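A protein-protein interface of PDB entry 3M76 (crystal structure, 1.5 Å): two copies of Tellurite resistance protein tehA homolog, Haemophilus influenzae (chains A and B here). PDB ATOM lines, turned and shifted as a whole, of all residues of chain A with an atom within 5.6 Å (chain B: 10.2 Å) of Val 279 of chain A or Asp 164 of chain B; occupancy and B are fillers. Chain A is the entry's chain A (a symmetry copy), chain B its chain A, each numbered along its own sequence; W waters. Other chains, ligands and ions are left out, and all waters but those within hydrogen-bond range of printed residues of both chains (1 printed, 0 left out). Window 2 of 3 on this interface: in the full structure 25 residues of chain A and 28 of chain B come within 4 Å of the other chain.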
ATOM      1  N   VAL A 223     -33.243   0.159 -15.043  1.00  0.00           N
ATOM      2  CA  VAL A 223     -32.129   0.362 -15.948  1.00  0.00           C
ATOM      3  C   VAL A 223     -31.989   1.842 -16.268  1.00  0.00           C
ATOM      4  O   VAL A 223     -32.651   2.408 -17.171  1.00  0.00           O
ATOM      5  CB  VAL A 223     -32.291  -0.425 -17.240  1.00  0.00           C
ATOM      6  CG1 VAL A 223     -31.084  -0.186 -18.165  1.00  0.00           C
ATOM      7  CG2 VAL A 223     -32.415  -1.904 -16.889  1.00  0.00           C
ATOM      8  N   LYS A 228     -26.442   1.993 -17.652  1.00  0.00           N
ATOM      9  CA  LYS A 228     -25.996   2.068 -19.037  1.00  0.00           C
ATOM     10  C   LYS A 228     -24.512   2.437 -19.129  1.00  0.00           C
ATOM     11  O   LYS A 228     -23.761   1.873 -19.925  1.00  0.00           O
ATOM     12  CB  LYS A 228     -26.848   3.058 -19.827  1.00  0.00           C
ATOM     13  CG  LYS A 228     -28.316   2.655 -19.953  1.00  0.00           C
ATOM     14  CD  LYS A 228     -29.164   3.867 -20.509  1.00  0.00           C
ATOM     15  CE  LYS A 228     -30.605   3.626 -20.241  1.00  0.00           C
ATOM     16  NZ  LYS A 228     -31.424   4.811 -20.662  1.00  0.00           N
ATOM     17  N   TRP A 231     -22.498  -0.691 -18.289  1.00  0.00           N
ATOM     18  CA  TRP A 231     -22.484  -1.602 -19.403  1.00  0.00           C
ATOM     19  C   TRP A 231     -21.529  -1.143 -20.472  1.00  0.00           C
ATOM     20  O   TRP A 231     -20.834  -1.992 -21.089  1.00  0.00           O
ATOM     21  CB  TRP A 231     -23.893  -1.767 -19.986  1.00  0.00           C
ATOM     22  CG  TRP A 231     -24.445  -3.135 -19.900  1.00  0.00           C
ATOM     23  CD1 TRP A 231     -24.160  -4.063 -18.956  1.00  0.00           C
ATOM     24  CD2 TRP A 231     -25.383  -3.721 -20.787  1.00  0.00           C
ATOM     25  NE1 TRP A 231     -24.855  -5.187 -19.193  1.00  0.00           N
ATOM     26  CE2 TRP A 231     -25.612  -5.021 -20.327  1.00  0.00           C
ATOM     27  CE3 TRP A 231     -26.050  -3.268 -21.914  1.00  0.00           C
ATOM     28  CZ2 TRP A 231     -26.502  -5.901 -20.982  1.00  0.00           C
ATOM     29  CZ3 TRP A 231     -26.936  -4.133 -22.554  1.00  0.00           C
ATOM     30  CH2 TRP A 231     -27.126  -5.428 -22.079  1.00  0.00           C
ATOM     31  N   PHE A 274     -31.680  -5.588 -18.578  1.00  0.00           N
ATOM     32  CA  PHE A 274     -31.787  -4.685 -19.713  1.00  0.00           C
ATOM     33  C   PHE A 274     -32.933  -5.095 -20.617  1.00  0.00           C
ATOM     34  O   PHE A 274     -33.748  -4.289 -21.008  1.00  0.00           O
ATOM     35  CB  PHE A 274     -30.463  -4.577 -20.504  1.00  0.00           C
ATOM     36  CG  PHE A 274     -29.466  -3.588 -19.896  1.00  0.00           C
ATOM     37  CD1 PHE A 274     -28.784  -3.849 -18.744  1.00  0.00           C
ATOM     38  CD2 PHE A 274     -29.244  -2.401 -20.527  1.00  0.00           C
ATOM     39  CE1 PHE A 274     -27.877  -2.904 -18.205  1.00  0.00           C
ATOM     40  CE2 PHE A 274     -28.359  -1.482 -20.013  1.00  0.00           C
ATOM     41  CZ  PHE A 274     -27.674  -1.742 -18.856  1.00  0.00           C
ATOM     42  N   TYR A 275     -33.027  -6.382 -20.884  1.00  0.00           N
ATOM     43  CA  TYR A 275     -34.105  -6.885 -21.729  1.00  0.00           C
ATOM     44  C   TYR A 275     -35.468  -6.603 -21.095  1.00  0.00           C
ATOM     45  O   TYR A 275     -36.371  -6.104 -21.764  1.00  0.00           O
ATOM     46  CB  TYR A 275     -33.922  -8.370 -22.024  1.00  0.00           C
ATOM     47  CG  TYR A 275     -34.828  -8.848 -23.140  1.00  0.00           C
ATOM     48  CD1 TYR A 275     -34.410  -8.792 -24.468  1.00  0.00           C
ATOM     49  CD2 TYR A 275     -36.104  -9.292 -22.875  1.00  0.00           C
ATOM     50  CE1 TYR A 275     -35.227  -9.190 -25.499  1.00  0.00           C
ATOM     51  CE2 TYR A 275     -36.937  -9.698 -23.917  1.00  0.00           C
ATOM     52  CZ  TYR A 275     -36.496  -9.645 -25.218  1.00  0.00           C
ATOM     53  OH  TYR A 275     -37.311 -10.042 -26.269  1.00  0.00           O
ATOM     54  N   GLY A 277     -36.249  -4.364 -19.098  1.00  0.00           N
ATOM     55  CA  GLY A 277     -36.456  -2.930 -19.093  1.00  0.00           C
ATOM     56  C   GLY A 277     -36.606  -2.304 -20.470  1.00  0.00           C
ATOM     57  O   GLY A 277     -36.767  -1.081 -20.620  1.00  0.00           O
ATOM     58  N   ASN A 278     -36.574  -3.151 -21.498  1.00  0.00           N
ATOM     59  CA  ASN A 278     -36.636  -2.689 -22.865  1.00  0.00           C
ATOM     60  C   ASN A 278     -35.560  -1.635 -23.168  1.00  0.00           C
ATOM     61  O   ASN A 278     -35.834  -0.608 -23.798  1.00  0.00           O
ATOM     62  CB  ASN A 278     -38.028  -2.143 -23.259  1.00  0.00           C
ATOM     63  CG  ASN A 278     -38.181  -1.977 -24.765  1.00  0.00           C
ATOM     64  OD1 ASN A 278     -37.513  -2.663 -25.539  1.00  0.00           O
ATOM     65  ND2 ASN A 278     -39.100  -1.094 -25.184  1.00  0.00           N
ATOM     66  N   VAL A 279     -34.343  -1.943 -22.778  1.00  0.00           N
ATOM     67  CA  VAL A 279     -33.183  -1.126 -23.101  1.00  0.00           C
ATOM     68  C   VAL A 279     -32.196  -2.007 -23.857  1.00  0.00           C
ATOM     69  O   VAL A 279     -31.778  -3.053 -23.363  1.00  0.00           O
ATOM     70  CB  VAL A 279     -32.493  -0.570 -21.820  1.00  0.00           C
ATOM     71  CG1 VAL A 279     -31.239   0.200 -22.212  1.00  0.00           C
ATOM     72  CG2 VAL A 279     -33.453   0.319 -21.032  1.00  0.00           C
ATOM     73  N   LEU A 280     -31.848  -1.595 -25.065  1.00  0.00           N
ATOM     74  CA  LEU A 280     -30.843  -2.297 -25.857  1.00  0.00           C
ATOM     75  C   LEU A 280     -31.142  -3.790 -25.903  1.00  0.00           C
ATOM     76  O   LEU A 280     -30.295  -4.631 -25.608  1.00  0.00           O
ATOM     77  CB  LEU A 280     -29.440  -2.012 -25.306  1.00  0.00           C
ATOM     78  CG  LEU A 280     -29.077  -0.530 -25.342  1.00  0.00           C
ATOM     79  CD1 LEU A 280     -27.854  -0.282 -24.455  1.00  0.00           C
ATOM     80  CD2 LEU A 280     -28.860  -0.082 -26.766  1.00  0.00           C
ATOM     81  N   GLN A 281     -32.359  -4.150 -26.290  1.00  0.00           N
ATOM     82  CA  GLN A 281     -32.711  -5.552 -26.280  1.00  0.00           C
ATOM     83  C   GLN A 281     -31.868  -6.433 -27.185  1.00  0.00           C
ATOM     84  O   GLN A 281     -31.621  -7.592 -26.869  1.00  0.00           O
ATOM     85  CB  GLN A 281     -34.201  -5.717 -26.604  1.00  0.00           C
ATOM     86  CG  GLN A 281     -35.124  -5.232 -25.510  1.00  0.00           C
ATOM     87  CD  GLN A 281     -36.560  -5.741 -25.683  1.00  0.00           C
ATOM     88  OE1 GLN A 281     -37.066  -5.827 -26.812  1.00  0.00           O
ATOM     89  NE2 GLN A 281     -37.205  -6.109 -24.573  1.00  0.00           N
ATOM     90  N   SER A 284     -28.702  -7.050 -25.549  1.00  0.00           N
ATOM     91  CA  SER A 284     -28.986  -7.951 -24.440  1.00  0.00           C
ATOM     92  C   SER A 284     -29.024  -9.406 -24.874  1.00  0.00           C
ATOM     93  O   SER A 284     -28.472 -10.297 -24.219  1.00  0.00           O
ATOM     94  CB  SER A 284     -30.310  -7.569 -23.777  1.00  0.00           C
ATOM     95  OG  SER A 284     -30.258  -6.265 -23.193  1.00  0.00           O
ATOM     96  N   TRP B 110     -20.910   7.078 -38.404  1.00  0.00           N
ATOM     97  CA  TRP B 110     -20.662   5.661 -38.236  1.00  0.00           C
ATOM     98  C   TRP B 110     -19.240   5.269 -38.619  1.00  0.00           C
ATOM     99  O   TRP B 110     -18.632   4.416 -37.969  1.00  0.00           O
ATOM    100  CB  TRP B 110     -21.659   4.802 -39.013  1.00  0.00           C
ATOM    101  CG  TRP B 110     -23.004   4.733 -38.373  1.00  0.00           C
ATOM    102  CD1 TRP B 110     -24.167   5.272 -38.865  1.00  0.00           C
ATOM    103  CD2 TRP B 110     -23.342   4.158 -37.110  1.00  0.00           C
ATOM    104  NE1 TRP B 110     -25.199   5.034 -38.005  1.00  0.00           N
ATOM    105  CE2 TRP B 110     -24.734   4.350 -36.920  1.00  0.00           C
ATOM    106  CE3 TRP B 110     -22.625   3.448 -36.146  1.00  0.00           C
ATOM    107  CZ2 TRP B 110     -25.411   3.884 -35.786  1.00  0.00           C
ATOM    108  CZ3 TRP B 110     -23.310   2.988 -35.011  1.00  0.00           C
ATOM    109  CH2 TRP B 110     -24.687   3.199 -34.860  1.00  0.00           C
ATOM    110  N   SER B 153     -18.174   9.758 -30.029  1.00  0.00           N
ATOM    111  CA  SER B 153     -19.186   8.802 -30.495  1.00  0.00           C
ATOM    112  C   SER B 153     -20.487   8.937 -29.726  1.00  0.00           C
ATOM    113  O   SER B 153     -21.564   8.871 -30.317  1.00  0.00           O
ATOM    114  CB  SER B 153     -18.703   7.359 -30.385  1.00  0.00           C
ATOM    115  OG  SER B 153     -17.713   7.078 -31.352  1.00  0.00           O
ATOM    116  N   ALA B 154     -20.409   9.127 -28.422  1.00  0.00           N
ATOM    117  CA  ALA B 154     -21.619   9.239 -27.605  1.00  0.00           C
ATOM    118  C   ALA B 154     -22.498  10.386 -28.080  1.00  0.00           C
ATOM    119  O   ALA B 154     -23.705  10.227 -28.274  1.00  0.00           O
ATOM    120  CB  ALA B 154     -21.246   9.427 -26.135  1.00  0.00           C
ATOM    121  N   SER B 155     -21.894  11.556 -28.236  1.00  0.00           N
ATOM    122  CA  SER B 155     -22.689  12.697 -28.620  1.00  0.00           C
ATOM    123  C   SER B 155     -23.163  12.608 -30.059  1.00  0.00           C
ATOM    124  O   SER B 155     -24.307  13.032 -30.362  1.00  0.00           O
ATOM    125  CB  SER B 155     -21.959  14.014 -28.363  1.00  0.00           C
ATOM    126  OG  SER B 155     -20.682  14.003 -28.984  1.00  0.00           O
ATOM    127  N   SER B 156     -22.357  12.047 -30.942  1.00  0.00           N
ATOM    128  CA  SER B 156     -22.768  11.943 -32.356  1.00  0.00           C
ATOM    129  C   SER B 156     -23.881  10.937 -32.518  1.00  0.00           C
ATOM    130  O   SER B 156     -24.802  11.135 -33.307  1.00  0.00           O
ATOM    131  CB  SER B 156     -21.570  11.545 -33.207  1.00  0.00           C
ATOM    132  OG  SER B 156     -20.560  12.530 -33.112  1.00  0.00           O
ATOM    133  N   LEU B 157     -23.813   9.828 -31.793  1.00  0.00           N
ATOM    134  CA  LEU B 157     -24.877   8.823 -31.858  1.00  0.00           C
ATOM    135  C   LEU B 157     -26.165   9.389 -31.278  1.00  0.00           C
ATOM    136  O   LEU B 157     -27.261   9.115 -31.811  1.00  0.00           O
ATOM    137  CB  LEU B 157     -24.438   7.524 -31.145  1.00  0.00           C
ATOM    138  CG  LEU B 157     -23.425   6.721 -31.948  1.00  0.00           C
ATOM    139  CD1 LEU B 157     -22.951   5.552 -31.072  1.00  0.00           C
ATOM    140  CD2 LEU B 157     -23.904   6.255 -33.241  1.00  0.00           C
ATOM    141  N   ALA B 158     -26.069  10.209 -30.236  1.00  0.00           N
ATOM    142  CA  ALA B 158     -27.274  10.824 -29.655  1.00  0.00           C
ATOM    143  C   ALA B 158     -27.929  11.773 -30.684  1.00  0.00           C
ATOM    144  O   ALA B 158     -29.155  11.833 -30.819  1.00  0.00           O
ATOM    145  CB  ALA B 158     -26.938  11.588 -28.372  1.00  0.00           C
ATOM    146  N   LEU B 159     -27.102  12.481 -31.437  1.00  0.00           N
ATOM    147  CA  LEU B 159     -27.610  13.381 -32.487  1.00  0.00           C
ATOM    148  C   LEU B 159     -28.466  12.601 -33.494  1.00  0.00           C
ATOM    149  O   LEU B 159     -29.522  13.099 -33.984  1.00  0.00           O
ATOM    150  CB  LEU B 159     -26.439  14.053 -33.211  1.00  0.00           C
ATOM    151  CG  LEU B 159     -26.776  14.970 -34.388  1.00  0.00           C
ATOM    152  CD1 LEU B 159     -27.616  16.179 -33.881  1.00  0.00           C
ATOM    153  CD2 LEU B 159     -25.527  15.442 -35.088  1.00  0.00           C
ATOM    154  N   LEU B 160     -28.031  11.371 -33.797  1.00  0.00           N
ATOM    155  CA  LEU B 160     -28.735  10.490 -34.718  1.00  0.00           C
ATOM    156  C   LEU B 160     -29.952   9.808 -34.099  1.00  0.00           C
ATOM    157  O   LEU B 160     -30.668   9.087 -34.797  1.00  0.00           O
ATOM    158  CB  LEU B 160     -27.804   9.403 -35.258  1.00  0.00           C
ATOM    159  CG  LEU B 160     -26.610   9.867 -36.071  1.00  0.00           C
ATOM    160  CD1 LEU B 160     -25.744   8.686 -36.464  1.00  0.00           C
ATOM    161  CD2 LEU B 160     -27.076  10.690 -37.268  1.00  0.00           C
ATOM    162  N   GLY B 161     -30.167  10.017 -32.799  1.00  0.00           N
ATOM    163  CA  GLY B 161     -31.298   9.423 -32.079  1.00  0.00           C
ATOM    164  C   GLY B 161     -30.986   8.149 -31.315  1.00  0.00           C
ATOM    165  O   GLY B 161     -31.881   7.549 -30.767  1.00  0.00           O
ATOM    166  N   TYR B 162     -29.723   7.732 -31.289  1.00  0.00           N
ATOM    167  CA  TYR B 162     -29.342   6.495 -30.608  1.00  0.00           C
ATOM    168  C   TYR B 162     -28.855   6.837 -29.189  1.00  0.00           C
ATOM    169  O   TYR B 162     -27.651   6.740 -28.903  1.00  0.00           O
ATOM    170  CB  TYR B 162     -28.241   5.767 -31.389  1.00  0.00           C
ATOM    171  CG  TYR B 162     -28.651   5.323 -32.770  1.00  0.00           C
ATOM    172  CD1 TYR B 162     -29.366   4.139 -32.951  1.00  0.00           C
ATOM    173  CD2 TYR B 162     -28.281   6.038 -33.890  1.00  0.00           C
ATOM    174  CE1 TYR B 162     -29.750   3.726 -34.216  1.00  0.00           C
ATOM    175  CE2 TYR B 162     -28.690   5.642 -35.159  1.00  0.00           C
ATOM    176  CZ  TYR B 162     -29.404   4.486 -35.300  1.00  0.00           C
ATOM    177  OH  TYR B 162     -29.805   4.032 -36.552  1.00  0.00           O
ATOM    178  N   HIS B 163     -29.756   7.272 -28.309  1.00  0.00           N
ATOM    179  CA  HIS B 163     -29.348   7.749 -27.002  1.00  0.00           C
ATOM    180  C   HIS B 163     -28.789   6.639 -26.132  1.00  0.00           C
ATOM    181  O   HIS B 163     -27.781   6.861 -25.465  1.00  0.00           O
ATOM    182  CB  HIS B 163     -30.504   8.441 -26.285  1.00  0.00           C
ATOM    183  CG  HIS B 163     -30.966   9.667 -26.984  1.00  0.00           C
ATOM    184  ND1 HIS B 163     -31.914   9.613 -27.984  1.00  0.00           N
ATOM    185  CD2 HIS B 163     -30.598  10.970 -26.857  1.00  0.00           C
ATOM    186  CE1 HIS B 163     -32.120  10.840 -28.437  1.00  0.00           C
ATOM    187  NE2 HIS B 163     -31.332  11.678 -27.787  1.00  0.00           N
ATOM    188  N   ASP B 164     -29.432   5.475 -26.093  1.00  0.00           N
ATOM    189  CA  ASP B 164     -28.946   4.383 -25.227  1.00  0.00           C
ATOM    190  C   ASP B 164     -27.619   3.837 -25.710  1.00  0.00           C
ATOM    191  O   ASP B 164     -26.735   3.629 -24.890  1.00  0.00           O
ATOM    192  CB  ASP B 164     -30.004   3.294 -25.079  1.00  0.00           C
ATOM    193  CG  ASP B 164     -31.164   3.733 -24.224  1.00  0.00           C
ATOM    194  OD1 ASP B 164     -31.027   4.716 -23.452  1.00  0.00           O
ATOM    195  OD2 ASP B 164     -32.214   3.065 -24.331  1.00  0.00           O
ATOM    196  N   LEU B 165     -27.412   3.681 -27.006  1.00  0.00           N
ATOM    197  CA  LEU B 165     -26.087   3.346 -27.531  1.00  0.00           C
ATOM    198  C   LEU B 165     -25.093   4.435 -27.164  1.00  0.00           C
ATOM    199  O   LEU B 165     -23.943   4.158 -26.783  1.00  0.00           O
ATOM    200  CB  LEU B 165     -26.163   3.216 -29.047  1.00  0.00           C
ATOM    201  CG  LEU B 165     -25.567   2.006 -29.714  1.00  0.00           C
ATOM    202  CD1 LEU B 165     -25.236   2.328 -31.161  1.00  0.00           C
ATOM    203  CD2 LEU B 165     -24.427   1.293 -29.028  1.00  0.00           C
ATOM    204  N   GLY B 166     -25.515   5.696 -27.272  1.00  0.00           N
ATOM    205  CA  GLY B 166     -24.661   6.804 -26.873  1.00  0.00           C
ATOM    206  C   GLY B 166     -24.209   6.680 -25.429  1.00  0.00           C
ATOM    207  O   GLY B 166     -23.053   6.986 -25.112  1.00  0.00           O
ATOM    208  N   TYR B 167     -25.114   6.292 -24.533  1.00  0.00           N
ATOM    209  CA  TYR B 167     -24.745   6.139 -23.133  1.00  0.00           C
ATOM    210  C   TYR B 167     -23.675   5.074 -22.946  1.00  0.00           C
ATOM    211  O   TYR B 167     -22.852   5.197 -22.041  1.00  0.00           O
ATOM    212  CB  TYR B 167     -25.924   5.840 -22.220  1.00  0.00           C
ATOM    213  CG  TYR B 167     -26.698   7.048 -21.746  1.00  0.00           C
ATOM    214  CD1 TYR B 167     -28.023   7.204 -22.063  1.00  0.00           C
ATOM    215  CD2 TYR B 167     -26.105   8.030 -20.960  1.00  0.00           C
ATOM    216  CE1 TYR B 167     -28.746   8.313 -21.596  1.00  0.00           C
ATOM    217  CE2 TYR B 167     -26.835   9.118 -20.503  1.00  0.00           C
ATOM    218  CZ  TYR B 167     -28.145   9.237 -20.816  1.00  0.00           C
ATOM    219  OH  TYR B 167     -28.861  10.372 -20.369  1.00  0.00           O
ATOM    220  N   LEU B 168     -23.681   4.029 -23.766  1.00  0.00           N
ATOM    221  CA  LEU B 168     -22.632   3.008 -23.649  1.00  0.00           C
ATOM    222  C   LEU B 168     -21.264   3.629 -23.965  1.00  0.00           C
ATOM    223  O   LEU B 168     -20.300   3.463 -23.228  1.00  0.00           O
ATOM    224  CB  LEU B 168     -22.858   1.837 -24.581  1.00  0.00           C
ATOM    225  CG  LEU B 168     -24.112   0.983 -24.449  1.00  0.00           C
ATOM    226  CD1 LEU B 168     -24.143  -0.190 -25.390  1.00  0.00           C
ATOM    227  CD2 LEU B 168     -24.214   0.520 -23.109  1.00  0.00           C
ATOM    228  N   PHE B 169     -21.172   4.353 -25.075  1.00  0.00           N
ATOM    229  CA  PHE B 169     -19.925   5.023 -25.419  1.00  0.00           C
ATOM    230  C   PHE B 169     -19.557   6.038 -24.353  1.00  0.00           C
ATOM    231  O   PHE B 169     -18.377   6.212 -24.032  1.00  0.00           O
ATOM    232  CB  PHE B 169     -20.002   5.654 -26.794  1.00  0.00           C
ATOM    233  CG  PHE B 169     -19.867   4.635 -27.918  1.00  0.00           C
ATOM    234  CD1 PHE B 169     -18.609   4.260 -28.356  1.00  0.00           C
ATOM    235  CD2 PHE B 169     -20.983   4.050 -28.509  1.00  0.00           C
ATOM    236  CE1 PHE B 169     -18.459   3.342 -29.364  1.00  0.00           C
ATOM    237  CE2 PHE B 169     -20.807   3.102 -29.512  1.00  0.00           C
ATOM    238  CZ  PHE B 169     -19.579   2.777 -29.939  1.00  0.00           C
ATOM    239  N   PHE B 170     -20.558   6.763 -23.844  1.00  0.00           N
ATOM    240  CA  PHE B 170     -20.324   7.733 -22.806  1.00  0.00           C
ATOM    241  C   PHE B 170     -19.691   7.109 -21.565  1.00  0.00           C
ATOM    242  O   PHE B 170     -18.686   7.621 -21.023  1.00  0.00           O
ATOM    243  CB  PHE B 170     -21.634   8.422 -22.423  1.00  0.00           C
ATOM    244  CG  PHE B 170     -21.459   9.438 -21.313  1.00  0.00           C
ATOM    245  CD1 PHE B 170     -20.903  10.685 -21.551  1.00  0.00           C
ATOM    246  CD2 PHE B 170     -21.759   9.110 -20.012  1.00  0.00           C
ATOM    247  CE1 PHE B 170     -20.641  11.546 -20.526  1.00  0.00           C
ATOM    248  CE2 PHE B 170     -21.543  10.012 -18.979  1.00  0.00           C
ATOM    249  CZ  PHE B 170     -20.968  11.204 -19.224  1.00  0.00           C
ATOM    250  N   GLY B 171     -20.245   5.985 -21.137  1.00  0.00           N
ATOM    251  CA  GLY B 171     -19.716   5.317 -19.983  1.00  0.00           C
ATOM    252  C   GLY B 171     -18.323   4.767 -20.186  1.00  0.00           C
ATOM    253  O   GLY B 171     -17.452   4.819 -19.288  1.00  0.00           O
ATOM    254  N   ALA B 172     -18.062   4.236 -21.368  1.00  0.00           N
ATOM    255  CA  ALA B 172     -16.722   3.772 -21.725  1.00  0.00           C
ATOM    256  C   ALA B 172     -15.733   4.922 -21.586  1.00  0.00           C
ATOM    257  O   ALA B 172     -14.671   4.774 -20.978  1.00  0.00           O
ATOM    258  CB  ALA B 172     -16.720   3.214 -23.119  1.00  0.00           C
ATOM    259  N   SER B 217     -25.498  16.308 -24.370  1.00  0.00           N
ATOM    260  CA  SER B 217     -26.005  15.929 -25.684  1.00  0.00           C
ATOM    261  C   SER B 217     -26.914  14.717 -25.640  1.00  0.00           C
ATOM    262  O   SER B 217     -27.905  14.621 -26.387  1.00  0.00           O
ATOM    263  CB  SER B 217     -24.855  15.655 -26.655  1.00  0.00           C
ATOM    264  OG  SER B 217     -24.116  16.839 -26.850  1.00  0.00           O
ATOM    265  N   ILE B 218     -26.616  13.776 -24.779  1.00  0.00           N
ATOM    266  CA  ILE B 218     -27.393  12.562 -24.664  1.00  0.00           C
ATOM    267  C   ILE B 218     -28.628  12.744 -23.777  1.00  0.00           C
ATOM    268  O   ILE B 218     -29.674  12.143 -24.030  1.00  0.00           O
ATOM    269  CB  ILE B 218     -26.595  11.422 -24.105  1.00  0.00           C
ATOM    270  CG1 ILE B 218     -25.344  11.178 -24.906  1.00  0.00           C
ATOM    271  CG2 ILE B 218     -27.447  10.219 -24.009  1.00  0.00           C
ATOM    272  CD1 ILE B 218     -24.363  10.427 -24.082  1.00  0.00           C
ATOM    273  N   ASN B 219     -28.521  13.578 -22.748  1.00  0.00           N
ATOM    274  CA  ASN B 219     -29.592  13.676 -21.775  1.00  0.00           C
ATOM    275  C   ASN B 219     -30.544  14.808 -22.042  1.00  0.00           C
ATOM    276  O   ASN B 219     -31.281  15.209 -21.136  1.00  0.00           O
ATOM    277  CB  ASN B 219     -29.018  13.712 -20.367  1.00  0.00           C
ATOM    278  CG  ASN B 219     -28.709  15.064 -19.923  1.00  0.00           C
ATOM    279  OD1 ASN B 219     -28.589  15.970 -20.743  1.00  0.00           O
ATOM    280  ND2 ASN B 219     -28.589  15.246 -18.598  1.00  0.00           N
ATOM    281  N   HIS B 220     -30.590  15.290 -23.284  1.00  0.00           N
ATOM    282  CA  HIS B 220     -31.509  16.339 -23.699  1.00  0.00           C
ATOM    283  C   HIS B 220     -31.259  17.699 -23.042  1.00  0.00           C
ATOM    284  O   HIS B 220     -32.173  18.531 -22.836  1.00  0.00           O
ATOM    285  CB  HIS B 220     -32.972  15.884 -23.504  1.00  0.00           C
ATOM    286  CG  HIS B 220     -33.295  14.620 -24.233  1.00  0.00           C
ATOM    287  ND1 HIS B 220     -33.581  14.596 -25.585  1.00  0.00           N
ATOM    288  CD2 HIS B 220     -33.364  13.337 -23.812  1.00  0.00           C
ATOM    289  CE1 HIS B 220     -33.817  13.352 -25.959  1.00  0.00           C
ATOM    290  NE2 HIS B 220     -33.682  12.568 -24.904  1.00  0.00           N
HETATM  291  O   HOH W   1     -32.729   1.041 -26.057  1.00  0.00           O
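Of the 25 printed residues of chain B, 3 touch a printed residue of chain A. Hydrophobic or aromatic side chains of chain B that line the printed part of chain A: Tyr 167 and Leu 168. Of the 11 printed residues of chain A, 4 touch a printed residue of chain B. Printed residues of chain A that touch a printed residue of chain B: Lys 228, Trp 231, Val 279 and Leu 280. Hydrophobic or aromatic side chains of chain A within 4 Å of the printed part of chain B: Trp 231, Val 279 and Leu 280. Among the printed residues, Asp or Glu carboxylates within 4 Å of a Lys or Arg side-chain nitrogen of the other chain: Lys 228 of chain A with Asp 164 of chain B.
No position is printed for both chains. Of the 7 pairs that touch across the chains among the printed residues, none has its exchanged pair printed and touching as well.
The backbone NH (N) of Val 279 of chain A sits at hydrogen-bond distance from the backbone carbonyl oxygen (O) of Phe 274 of chain A. O of Leu 280 of chain A sits at hydrogen-bond distance from OG of Ser 284 of chain A (2.9 Å).
NZ of Lys 228 of chain A is in salt-bridge range of OD1 of Asp 164 of chain B (2.8 Å).
Among the printed residues, pairs that only touch across the chains: Lys 228 of chain A with Tyr 167 of chain B (3.8 Å), Lys 228 of chain A with Leu 168 of chain B (3.5 Å), Trp 231 of chain A with Leu 168 of chain B (3.9 Å), Val 279 of chain A with Asp 164 of chain B (3.7 Å), Leu 280 of chain A with Asp 164 of chain B (3.9 Å) and Leu 280 of chain A with Leu 168 of chain B (3.8 Å).
No residue of chain B comes within 4 Å of Gly 277 of chain A. Val 279 of chain A touches just one residue of chain B: Asp 164. Asp 164 of chain B touches three residues of chain A. Printed residues of chain A within 4 Å of Tyr 167 of chain B: Lys 228. Printed residues of chain A within 4 Å of Leu 168 of chain B: Lys 228 (3.5 Å), Trp 231 (3.9 Å) and Leu 280 (3.8 Å). The nearest residue of chain A that does not touch Asp 164 of chain B is Asn 278 of chain A (5.2 Å). The nearest printed residue of chain B that does not touch Trp 231 of chain A is Ala 172 of chain B (6.5 Å).
Water W1 lies within hydrogen-bond range of the side-chain carboxylate (OD2) of Asp 164 of chain B and the backbone NH (N) of Leu 280 of chain A.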
